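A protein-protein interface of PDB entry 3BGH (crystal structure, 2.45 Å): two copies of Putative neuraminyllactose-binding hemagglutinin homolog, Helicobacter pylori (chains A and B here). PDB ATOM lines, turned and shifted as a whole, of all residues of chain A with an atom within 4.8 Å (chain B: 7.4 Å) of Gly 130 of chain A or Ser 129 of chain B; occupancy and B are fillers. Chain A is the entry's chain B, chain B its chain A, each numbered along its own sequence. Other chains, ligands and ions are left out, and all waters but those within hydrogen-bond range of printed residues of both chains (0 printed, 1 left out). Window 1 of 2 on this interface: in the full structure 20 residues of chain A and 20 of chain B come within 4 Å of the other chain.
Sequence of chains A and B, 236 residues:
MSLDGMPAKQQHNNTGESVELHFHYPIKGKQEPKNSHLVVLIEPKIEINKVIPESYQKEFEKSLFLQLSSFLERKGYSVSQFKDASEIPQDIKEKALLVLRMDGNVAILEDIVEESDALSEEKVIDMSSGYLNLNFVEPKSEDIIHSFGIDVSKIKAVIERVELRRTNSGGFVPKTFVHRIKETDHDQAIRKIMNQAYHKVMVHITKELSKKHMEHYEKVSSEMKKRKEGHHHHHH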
ATOM      1  N   ASN A 105     -11.932  -7.697  -2.908  1.00  0.00           N
ATOM      2  CA  ASN A 105     -11.008  -8.802  -2.828  1.00  0.00           C
ATOM      3  C   ASN A 105     -10.506  -9.111  -1.435  1.00  0.00           C
ATOM      4  O   ASN A 105     -10.541  -8.247  -0.559  1.00  0.00           O
ATOM      5  CB  ASN A 105      -9.787  -8.527  -3.699  1.00  0.00           C
ATOM      6  CG  ASN A 105      -8.888  -7.513  -3.104  1.00  0.00           C
ATOM      7  OD1 ASN A 105      -9.185  -6.320  -3.149  1.00  0.00           O
ATOM      8  ND2 ASN A 105      -7.772  -7.963  -2.532  1.00  0.00           N
ATOM      9  N   VAL A 106     -10.005 -10.342  -1.273  1.00  0.00           N
ATOM     10  CA  VAL A 106      -9.334 -10.801  -0.075  1.00  0.00           C
ATOM     11  C   VAL A 106      -8.053 -11.426  -0.577  1.00  0.00           C
ATOM     12  O   VAL A 106      -8.107 -12.218  -1.493  1.00  0.00           O
ATOM     13  CB  VAL A 106     -10.114 -11.932   0.653  1.00  0.00           C
ATOM     14  CG1 VAL A 106      -9.389 -12.363   1.973  1.00  0.00           C
ATOM     15  CG2 VAL A 106     -11.588 -11.525   0.923  1.00  0.00           C
ATOM     16  N   ALA A 107      -6.919 -11.113   0.035  1.00  0.00           N
ATOM     17  CA  ALA A 107      -5.675 -11.776  -0.287  1.00  0.00           C
ATOM     18  C   ALA A 107      -4.985 -12.276   0.958  1.00  0.00           C
ATOM     19  O   ALA A 107      -5.145 -11.718   2.032  1.00  0.00           O
ATOM     20  CB  ALA A 107      -4.729 -10.827  -1.112  1.00  0.00           C
ATOM     21  N   SER A 128      -4.131 -11.278   6.144  1.00  0.00           N
ATOM     22  CA  SER A 128      -4.950 -10.811   5.028  1.00  0.00           C
ATOM     23  C   SER A 128      -4.663  -9.385   4.650  1.00  0.00           C
ATOM     24  O   SER A 128      -4.177  -8.570   5.452  1.00  0.00           O
ATOM     25  CB  SER A 128      -6.440 -10.894   5.400  1.00  0.00           C
ATOM     26  OG  SER A 128      -6.782 -10.064   6.524  1.00  0.00           O
ATOM     27  N   SER A 129      -4.974  -9.069   3.409  1.00  0.00           N
ATOM     28  CA  SER A 129      -5.197  -7.697   3.036  1.00  0.00           C
ATOM     29  C   SER A 129      -6.517  -7.766   2.334  1.00  0.00           C
ATOM     30  O   SER A 129      -7.077  -8.869   2.153  1.00  0.00           O
ATOM     31  CB  SER A 129      -4.082  -7.189   2.117  1.00  0.00           C
ATOM     32  OG  SER A 129      -4.179  -7.800   0.849  1.00  0.00           O
ATOM     33  N   GLY A 130      -7.035  -6.640   1.908  1.00  0.00           N
ATOM     34  CA  GLY A 130      -8.249  -6.663   1.111  1.00  0.00           C
ATOM     35  C   GLY A 130      -9.393  -5.811   1.652  1.00  0.00           C
ATOM     36  O   GLY A 130      -9.318  -5.213   2.723  1.00  0.00           O
ATOM     37  N   TYR A 131     -10.460  -5.755   0.866  1.00  0.00           N
ATOM     38  CA  TYR A 131     -11.514  -4.797   1.089  1.00  0.00           C
ATOM     39  C   TYR A 131     -12.724  -5.257   0.343  1.00  0.00           C
ATOM     40  O   TYR A 131     -12.621  -5.829  -0.757  1.00  0.00           O
ATOM     41  CB  TYR A 131     -11.084  -3.431   0.576  1.00  0.00           C
ATOM     42  CG  TYR A 131     -11.916  -2.268   1.077  1.00  0.00           C
ATOM     43  CD1 TYR A 131     -11.640  -1.650   2.313  1.00  0.00           C
ATOM     44  CD2 TYR A 131     -12.971  -1.764   0.308  1.00  0.00           C
ATOM     45  CE1 TYR A 131     -12.432  -0.545   2.781  1.00  0.00           C
ATOM     46  CE2 TYR A 131     -13.747  -0.697   0.738  1.00  0.00           C
ATOM     47  CZ  TYR A 131     -13.476  -0.087   1.965  1.00  0.00           C
ATOM     48  OH  TYR A 131     -14.253   0.969   2.357  1.00  0.00           O
ATOM     49  N   LEU A 132     -13.875  -5.016   0.943  1.00  0.00           N
ATOM     50  CA  LEU A 132     -15.146  -5.318   0.299  1.00  0.00           C
ATOM     51  C   LEU A 132     -15.996  -4.094   0.294  1.00  0.00           C
ATOM     52  O   LEU A 132     -16.210  -3.474   1.335  1.00  0.00           O
ATOM     53  CB  LEU A 132     -15.891  -6.419   1.051  1.00  0.00           C
ATOM     54  CG  LEU A 132     -15.584  -7.782   0.477  1.00  0.00           C
ATOM     55  CD1 LEU A 132     -14.217  -8.246   0.892  1.00  0.00           C
ATOM     56  CD2 LEU A 132     -16.638  -8.779   0.894  1.00  0.00           C
ATOM     57  N   ASP A 151     -13.398  -3.324   5.694  1.00  0.00           N
ATOM     58  CA  ASP A 151     -11.966  -3.608   5.620  1.00  0.00           C
ATOM     59  C   ASP A 151     -11.777  -5.024   6.145  1.00  0.00           C
ATOM     60  O   ASP A 151     -12.210  -5.349   7.271  1.00  0.00           O
ATOM     61  CB  ASP A 151     -11.235  -2.624   6.523  1.00  0.00           C
ATOM     62  CG  ASP A 151      -9.713  -2.726   6.435  1.00  0.00           C
ATOM     63  OD1 ASP A 151      -9.157  -3.579   5.697  1.00  0.00           O
ATOM     64  OD2 ASP A 151      -9.067  -1.908   7.121  1.00  0.00           O
ATOM     65  N   VAL A 152     -11.169  -5.884   5.337  1.00  0.00           N
ATOM     66  CA  VAL A 152     -10.939  -7.256   5.784  1.00  0.00           C
ATOM     67  C   VAL A 152      -9.467  -7.564   5.907  1.00  0.00           C
ATOM     68  O   VAL A 152      -9.077  -8.732   5.790  1.00  0.00           O
ATOM     69  CB  VAL A 152     -11.603  -8.310   4.892  1.00  0.00           C
ATOM     70  CG1 VAL A 152     -13.104  -8.096   4.854  1.00  0.00           C
ATOM     71  CG2 VAL A 152     -11.041  -8.284   3.468  1.00  0.00           C
ATOM     72  N   SER A 153      -8.651  -6.553   6.168  1.00  0.00           N
ATOM     73  CA  SER A 153      -7.204  -6.775   6.248  1.00  0.00           C
ATOM     74  C   SER A 153      -6.688  -6.928   7.682  1.00  0.00           C
ATOM     75  O   SER A 153      -7.359  -6.581   8.647  1.00  0.00           O
ATOM     76  CB  SER A 153      -6.465  -5.634   5.523  1.00  0.00           C
ATOM     77  OG  SER A 153      -6.606  -4.391   6.204  1.00  0.00           O
ATOM     78  N   ASN B  49      -4.859  -7.462  -8.899  1.00  0.00           N
ATOM     79  CA  ASN B  49      -6.210  -7.933  -9.208  1.00  0.00           C
ATOM     80  C   ASN B  49      -6.569  -7.640 -10.681  1.00  0.00           C
ATOM     81  O   ASN B  49      -5.774  -7.050 -11.406  1.00  0.00           O
ATOM     82  CB  ASN B  49      -7.239  -7.334  -8.237  1.00  0.00           C
ATOM     83  CG  ASN B  49      -7.563  -5.883  -8.542  1.00  0.00           C
ATOM     84  OD1 ASN B  49      -6.680  -5.084  -8.795  1.00  0.00           O
ATOM     85  ND2 ASN B  49      -8.829  -5.540  -8.490  1.00  0.00           N
ATOM     86  N   ILE B  52      -5.974  -4.354 -13.129  1.00  0.00           N
ATOM     87  CA  ILE B  52      -4.601  -3.876 -13.400  1.00  0.00           C
ATOM     88  C   ILE B  52      -3.876  -4.686 -14.531  1.00  0.00           C
ATOM     89  O   ILE B  52      -3.753  -5.889 -14.434  1.00  0.00           O
ATOM     90  CB  ILE B  52      -3.723  -3.909 -12.097  1.00  0.00           C
ATOM     91  CG1 ILE B  52      -4.321  -3.015 -11.015  1.00  0.00           C
ATOM     92  CG2 ILE B  52      -2.279  -3.495 -12.386  1.00  0.00           C
ATOM     93  CD1 ILE B  52      -3.705  -3.174  -9.589  1.00  0.00           C
ATOM     94  N   ASN B 105       0.734  -7.805  -2.598  1.00  0.00           N
ATOM     95  CA  ASN B 105      -0.277  -7.595  -3.616  1.00  0.00           C
ATOM     96  C   ASN B 105      -0.800  -6.222  -3.548  1.00  0.00           C
ATOM     97  O   ASN B 105      -0.749  -5.560  -2.494  1.00  0.00           O
ATOM     98  CB  ASN B 105      -1.478  -8.578  -3.452  1.00  0.00           C
ATOM     99  CG  ASN B 105      -2.433  -8.136  -2.369  1.00  0.00           C
ATOM    100  OD1 ASN B 105      -2.174  -8.352  -1.174  1.00  0.00           O
ATOM    101  ND2 ASN B 105      -3.520  -7.477  -2.766  1.00  0.00           N
ATOM    102  N   VAL B 106      -1.322  -5.788  -4.681  1.00  0.00           N
ATOM    103  CA  VAL B 106      -2.035  -4.532  -4.765  1.00  0.00           C
ATOM    104  C   VAL B 106      -3.259  -4.747  -5.632  1.00  0.00           C
ATOM    105  O   VAL B 106      -3.196  -5.410  -6.663  1.00  0.00           O
ATOM    106  CB  VAL B 106      -1.140  -3.336  -5.224  1.00  0.00           C
ATOM    107  CG1 VAL B 106      -0.582  -3.558  -6.590  1.00  0.00           C
ATOM    108  CG2 VAL B 106      -1.940  -2.031  -5.214  1.00  0.00           C
ATOM    109  N   ALA B 107      -4.395  -4.239  -5.178  1.00  0.00           N
ATOM    110  CA  ALA B 107      -5.636  -4.391  -5.896  1.00  0.00           C
ATOM    111  C   ALA B 107      -6.297  -3.042  -5.971  1.00  0.00           C
ATOM    112  O   ALA B 107      -6.144  -2.218  -5.078  1.00  0.00           O
ATOM    113  CB  ALA B 107      -6.519  -5.389  -5.202  1.00  0.00           C
ATOM    114  N   ILE B 108      -7.006  -2.808  -7.064  1.00  0.00           N
ATOM    115  CA  ILE B 108      -7.769  -1.590  -7.213  1.00  0.00           C
ATOM    116  C   ILE B 108      -9.289  -1.914  -7.273  1.00  0.00           C
ATOM    117  O   ILE B 108      -9.750  -2.789  -8.012  1.00  0.00           O
ATOM    118  CB  ILE B 108      -7.212  -0.740  -8.375  1.00  0.00           C
ATOM    119  CG1 ILE B 108      -5.870  -0.175  -7.914  1.00  0.00           C
ATOM    120  CG2 ILE B 108      -8.158   0.410  -8.743  1.00  0.00           C
ATOM    121  CD1 ILE B 108      -5.003   0.368  -8.949  1.00  0.00           C
ATOM    122  N   LEU B 109     -10.034  -1.253  -6.395  1.00  0.00           N
ATOM    123  CA  LEU B 109     -11.487  -1.323  -6.379  1.00  0.00           C
ATOM    124  C   LEU B 109     -12.028  -0.111  -7.104  1.00  0.00           C
ATOM    125  O   LEU B 109     -11.523   0.994  -6.970  1.00  0.00           O
ATOM    126  CB  LEU B 109     -11.994  -1.334  -4.954  1.00  0.00           C
ATOM    127  CG  LEU B 109     -11.881  -2.640  -4.170  1.00  0.00           C
ATOM    128  CD1 LEU B 109     -10.437  -3.068  -3.909  1.00  0.00           C
ATOM    129  CD2 LEU B 109     -12.597  -2.444  -2.879  1.00  0.00           C
ATOM    130  N   MET B 127     -10.078   3.049  -5.536  1.00  0.00           N
ATOM    131  CA  MET B 127      -9.313   2.974  -4.299  1.00  0.00           C
ATOM    132  C   MET B 127      -8.578   1.656  -4.215  1.00  0.00           C
ATOM    133  O   MET B 127      -9.146   0.610  -4.528  1.00  0.00           O
ATOM    134  CB  MET B 127     -10.241   3.122  -3.070  1.00  0.00           C
ATOM    135  CG  MET B 127      -9.499   3.232  -1.688  1.00  0.00           C
ATOM    136  SD  MET B 127     -10.584   3.387  -0.201  1.00  0.00           S
ATOM    137  CE  MET B 127     -11.236   1.766  -0.189  1.00  0.00           C
ATOM    138  N   SER B 128      -7.339   1.699  -3.744  1.00  0.00           N
ATOM    139  CA  SER B 128      -6.556   0.502  -3.605  1.00  0.00           C
ATOM    140  C   SER B 128      -6.728  -0.243  -2.280  1.00  0.00           C
ATOM    141  O   SER B 128      -7.163   0.308  -1.250  1.00  0.00           O
ATOM    142  CB  SER B 128      -5.108   0.881  -3.695  1.00  0.00           C
ATOM    143  OG  SER B 128      -4.795   1.504  -2.467  1.00  0.00           O
ATOM    144  N   SER B 129      -6.298  -1.497  -2.305  1.00  0.00           N
ATOM    145  CA  SER B 129      -6.030  -2.269  -1.101  1.00  0.00           C
ATOM    146  C   SER B 129      -4.737  -3.021  -1.388  1.00  0.00           C
ATOM    147  O   SER B 129      -4.213  -2.968  -2.506  1.00  0.00           O
ATOM    148  CB  SER B 129      -7.178  -3.242  -0.826  1.00  0.00           C
ATOM    149  OG  SER B 129      -7.140  -4.319  -1.741  1.00  0.00           O
ATOM    150  N   GLY B 130      -4.237  -3.738  -0.403  1.00  0.00           N
ATOM    151  CA  GLY B 130      -3.038  -4.520  -0.543  1.00  0.00           C
ATOM    152  C   GLY B 130      -1.991  -4.140   0.479  1.00  0.00           C
ATOM    153  O   GLY B 130      -2.203  -3.314   1.315  1.00  0.00           O
ATOM    154  N   TYR B 131      -0.835  -4.749   0.372  1.00  0.00           N
ATOM    155  CA  TYR B 131       0.102  -4.738   1.432  1.00  0.00           C
ATOM    156  C   TYR B 131       1.386  -5.433   0.923  1.00  0.00           C
ATOM    157  O   TYR B 131       1.330  -6.484   0.291  1.00  0.00           O
ATOM    158  CB  TYR B 131      -0.512  -5.470   2.655  1.00  0.00           C
ATOM    159  CG  TYR B 131       0.341  -5.428   3.890  1.00  0.00           C
ATOM    160  CD1 TYR B 131       0.126  -4.481   4.890  1.00  0.00           C
ATOM    161  CD2 TYR B 131       1.387  -6.342   4.064  1.00  0.00           C
ATOM    162  CE1 TYR B 131       0.943  -4.427   6.042  1.00  0.00           C
ATOM    163  CE2 TYR B 131       2.205  -6.313   5.229  1.00  0.00           C
ATOM    164  CZ  TYR B 131       1.959  -5.369   6.199  1.00  0.00           C
ATOM    165  OH  TYR B 131       2.774  -5.360   7.298  1.00  0.00           O
ATOM    166  N   ASP B 151       1.855  -1.006   4.063  1.00  0.00           N
ATOM    167  CA  ASP B 151       0.468  -0.990   3.694  1.00  0.00           C
ATOM    168  C   ASP B 151       0.293  -0.013   2.519  1.00  0.00           C
ATOM    169  O   ASP B 151       0.695   1.177   2.590  1.00  0.00           O
ATOM    170  CB  ASP B 151      -0.340  -0.509   4.899  1.00  0.00           C
ATOM    171  CG  ASP B 151      -1.834  -0.426   4.634  1.00  0.00           C
ATOM    172  OD1 ASP B 151      -2.329  -0.661   3.506  1.00  0.00           O
ATOM    173  OD2 ASP B 151      -2.541  -0.087   5.589  1.00  0.00           O
ATOM    174  N   VAL B 152      -0.332  -0.507   1.453  1.00  0.00           N
ATOM    175  CA  VAL B 152      -0.557   0.312   0.273  1.00  0.00           C
ATOM    176  C   VAL B 152      -2.056   0.451   0.004  1.00  0.00           C
ATOM    177  O   VAL B 152      -2.460   0.770  -1.094  1.00  0.00           O
ATOM    178  CB  VAL B 152       0.144  -0.296  -1.007  1.00  0.00           C
ATOM    179  CG1 VAL B 152       1.683  -0.185  -0.916  1.00  0.00           C
ATOM    180  CG2 VAL B 152      -0.352  -1.751  -1.300  1.00  0.00           C
ATOM    181  N   SER B 153      -2.888   0.204   1.001  1.00  0.00           N
ATOM    182  CA  SER B 153      -4.329   0.367   0.820  1.00  0.00           C
ATOM    183  C   SER B 153      -4.814   1.806   1.064  1.00  0.00           C
ATOM    184  O   SER B 153      -4.060   2.655   1.538  1.00  0.00           O
ATOM    185  CB  SER B 153      -5.048  -0.598   1.724  1.00  0.00           C
ATOM    186  OG  SER B 153      -5.020  -0.119   3.053  1.00  0.00           O
ATOM    187  N   LYS B 154      -6.078   2.071   0.742  1.00  0.00           N
ATOM    188  CA  LYS B 154      -6.697   3.420   0.888  1.00  0.00           C
ATOM    189  C   LYS B 154      -6.122   4.541   0.021  1.00  0.00           C
ATOM    190  O   LYS B 154      -6.409   5.722   0.251  1.00  0.00           O
ATOM    191  CB  LYS B 154      -6.779   3.876   2.363  1.00  0.00           C
ATOM    192  CG  LYS B 154      -7.408   2.868   3.296  1.00  0.00           C
ATOM    193  CD  LYS B 154      -8.910   2.940   3.316  1.00  0.00           C
ATOM    194  CE  LYS B 154      -9.472   2.474   4.696  1.00  0.00           C
ATOM    195  NZ  LYS B 154     -10.963   2.592   4.767  1.00  0.00           N
ATOM    196  N   ILE B 155      -5.331   4.197  -0.978  1.00  0.00           N
ATOM    197  CA  ILE B 155      -4.953   5.170  -1.990  1.00  0.00           C
ATOM    198  C   ILE B 155      -6.079   5.465  -3.013  1.00  0.00           C
ATOM    199  O   ILE B 155      -6.556   4.557  -3.697  1.00  0.00           O
ATOM    200  CB  ILE B 155      -3.623   4.772  -2.664  1.00  0.00           C
ATOM    201  CG1 ILE B 155      -2.509   4.711  -1.585  1.00  0.00           C
ATOM    202  CG2 ILE B 155      -3.274   5.777  -3.710  1.00  0.00           C
ATOM    203  CD1 ILE B 155      -1.135   4.321  -2.069  1.00  0.00           C
ATOM    204  N   ILE B 193      -2.967   5.786  -8.883  1.00  0.00           N
ATOM    205  CA  ILE B 193      -2.944   5.022  -7.657  1.00  0.00           C
ATOM    206  C   ILE B 193      -1.656   4.228  -7.531  1.00  0.00           C
ATOM    207  O   ILE B 193      -1.014   4.253  -6.469  1.00  0.00           O
ATOM    208  CB  ILE B 193      -4.210   4.120  -7.544  1.00  0.00           C
ATOM    209  CG1 ILE B 193      -5.423   5.005  -7.188  1.00  0.00           C
ATOM    210  CG2 ILE B 193      -3.990   2.976  -6.549  1.00  0.00           C
ATOM    211  CD1 ILE B 193      -6.794   4.363  -7.391  1.00  0.00           C
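Of the 18 printed residues of chain B, 8 touch a printed residue of chain A. Along chain A the printed residues that touch a printed residue of chain B span positions 105 to 131. Among the printed residues, no Asp or Glu carboxylate lies within 4 Å of a Lys or Arg side-chain nitrogen of the other chain.
Asn 105 of chain A touches Ala 107 of chain B, and with the chains exchanged Ala 107 of chain A touches Asn 105 of chain B. Asn 105 of chain A touches Ser 129 of chain B, and with the chains exchanged Ser 129 of chain A touches Asn 105 of chain B. Ser 129 of chain A touches Gly 130 of chain B, and with the chains exchanged Gly 130 of chain A touches Ser 129 of chain B. Ser 129 of chain A touches Tyr 131 of chain B, but with the chains exchanged Tyr 131 of chain A does not touch Ser 129 of chain B (4.2 Å).
Of the printed residues of chain B, Gly 130 of chain A touches Ser 129. Of the printed residues of chain B, Asn 105 of chain A touches Ala 107 (3.5 Å), Leu 109 (3.6 Å) and Ser 129 (3.2 Å). Of the printed residues of chain B, Ala 107 of chain A touches Asn 105. Printed residues of chain A within 4 Å of Ala 107 of chain B: Asn 105. Printed residues of chain B within 4 Å of Ser 129 of chain A: Asn 105, Gly 130 and Tyr 131. Printed residues of chain A within 4 Å of Met 127 of chain B: Tyr 131 (3.6 Å). The nearest printed residue of chain B that does not touch Ala 107 of chain A is Gly 130 of chain B (6.6 Å).
OG of Ser 129 of chain A sits at hydrogen-bond distance from OD1 of Asn 105 of chain B (2.9 Å). The side-chain hydroxyl (OG) of Ser 129 of chain B lies within hydrogen-bond range of the side-chain amide oxygen (OD1) of Asn 105 of chain A (3.2 Å).
Among the printed residues, pairs that only touch across the chains: Tyr 131 of chain A with Leu 109 of chain B, Asn 105 of chain A with Ala 107 of chain B, Ala 107 of chain A with Asn 105 of chain B, Asn 105 of chain A with Leu 109 of chain B, Tyr 131 of chain A with Met 127 of chain B, Ser 129 of chain A with Gly 130 of chain B, Gly 130 of chain A with Ser 129 of chain B, Tyr 131 of chain A with Lys 154 of chain B and Ser 129 of chain A with Tyr 131 of chain B.
O of Asn 105 of chain B sits at hydrogen-bond distance from N of Tyr 131 of chain B, 3.0 Å away. O of Met 127 of chain B is in hydrogen-bond range of N of Leu 109 of chain B (2.8 Å). O of Ser 128 of chain B is in hydrogen-bond range of N of Lys 154 of chain B (2.9 Å). The backbone NH (N) of Val 152 of chain B sits at hydrogen-bond distance from the backbone carbonyl oxygen (O) of Gly 130 of chain B (3.4 Å). O of Asn 105 of chain A sits at hydrogen-bond distance from N of Tyr 131 of chain A. O of Ala 107 of chain A lies within hydrogen-bond range of N of Ser 129 of chain A, at 3.0 Å.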
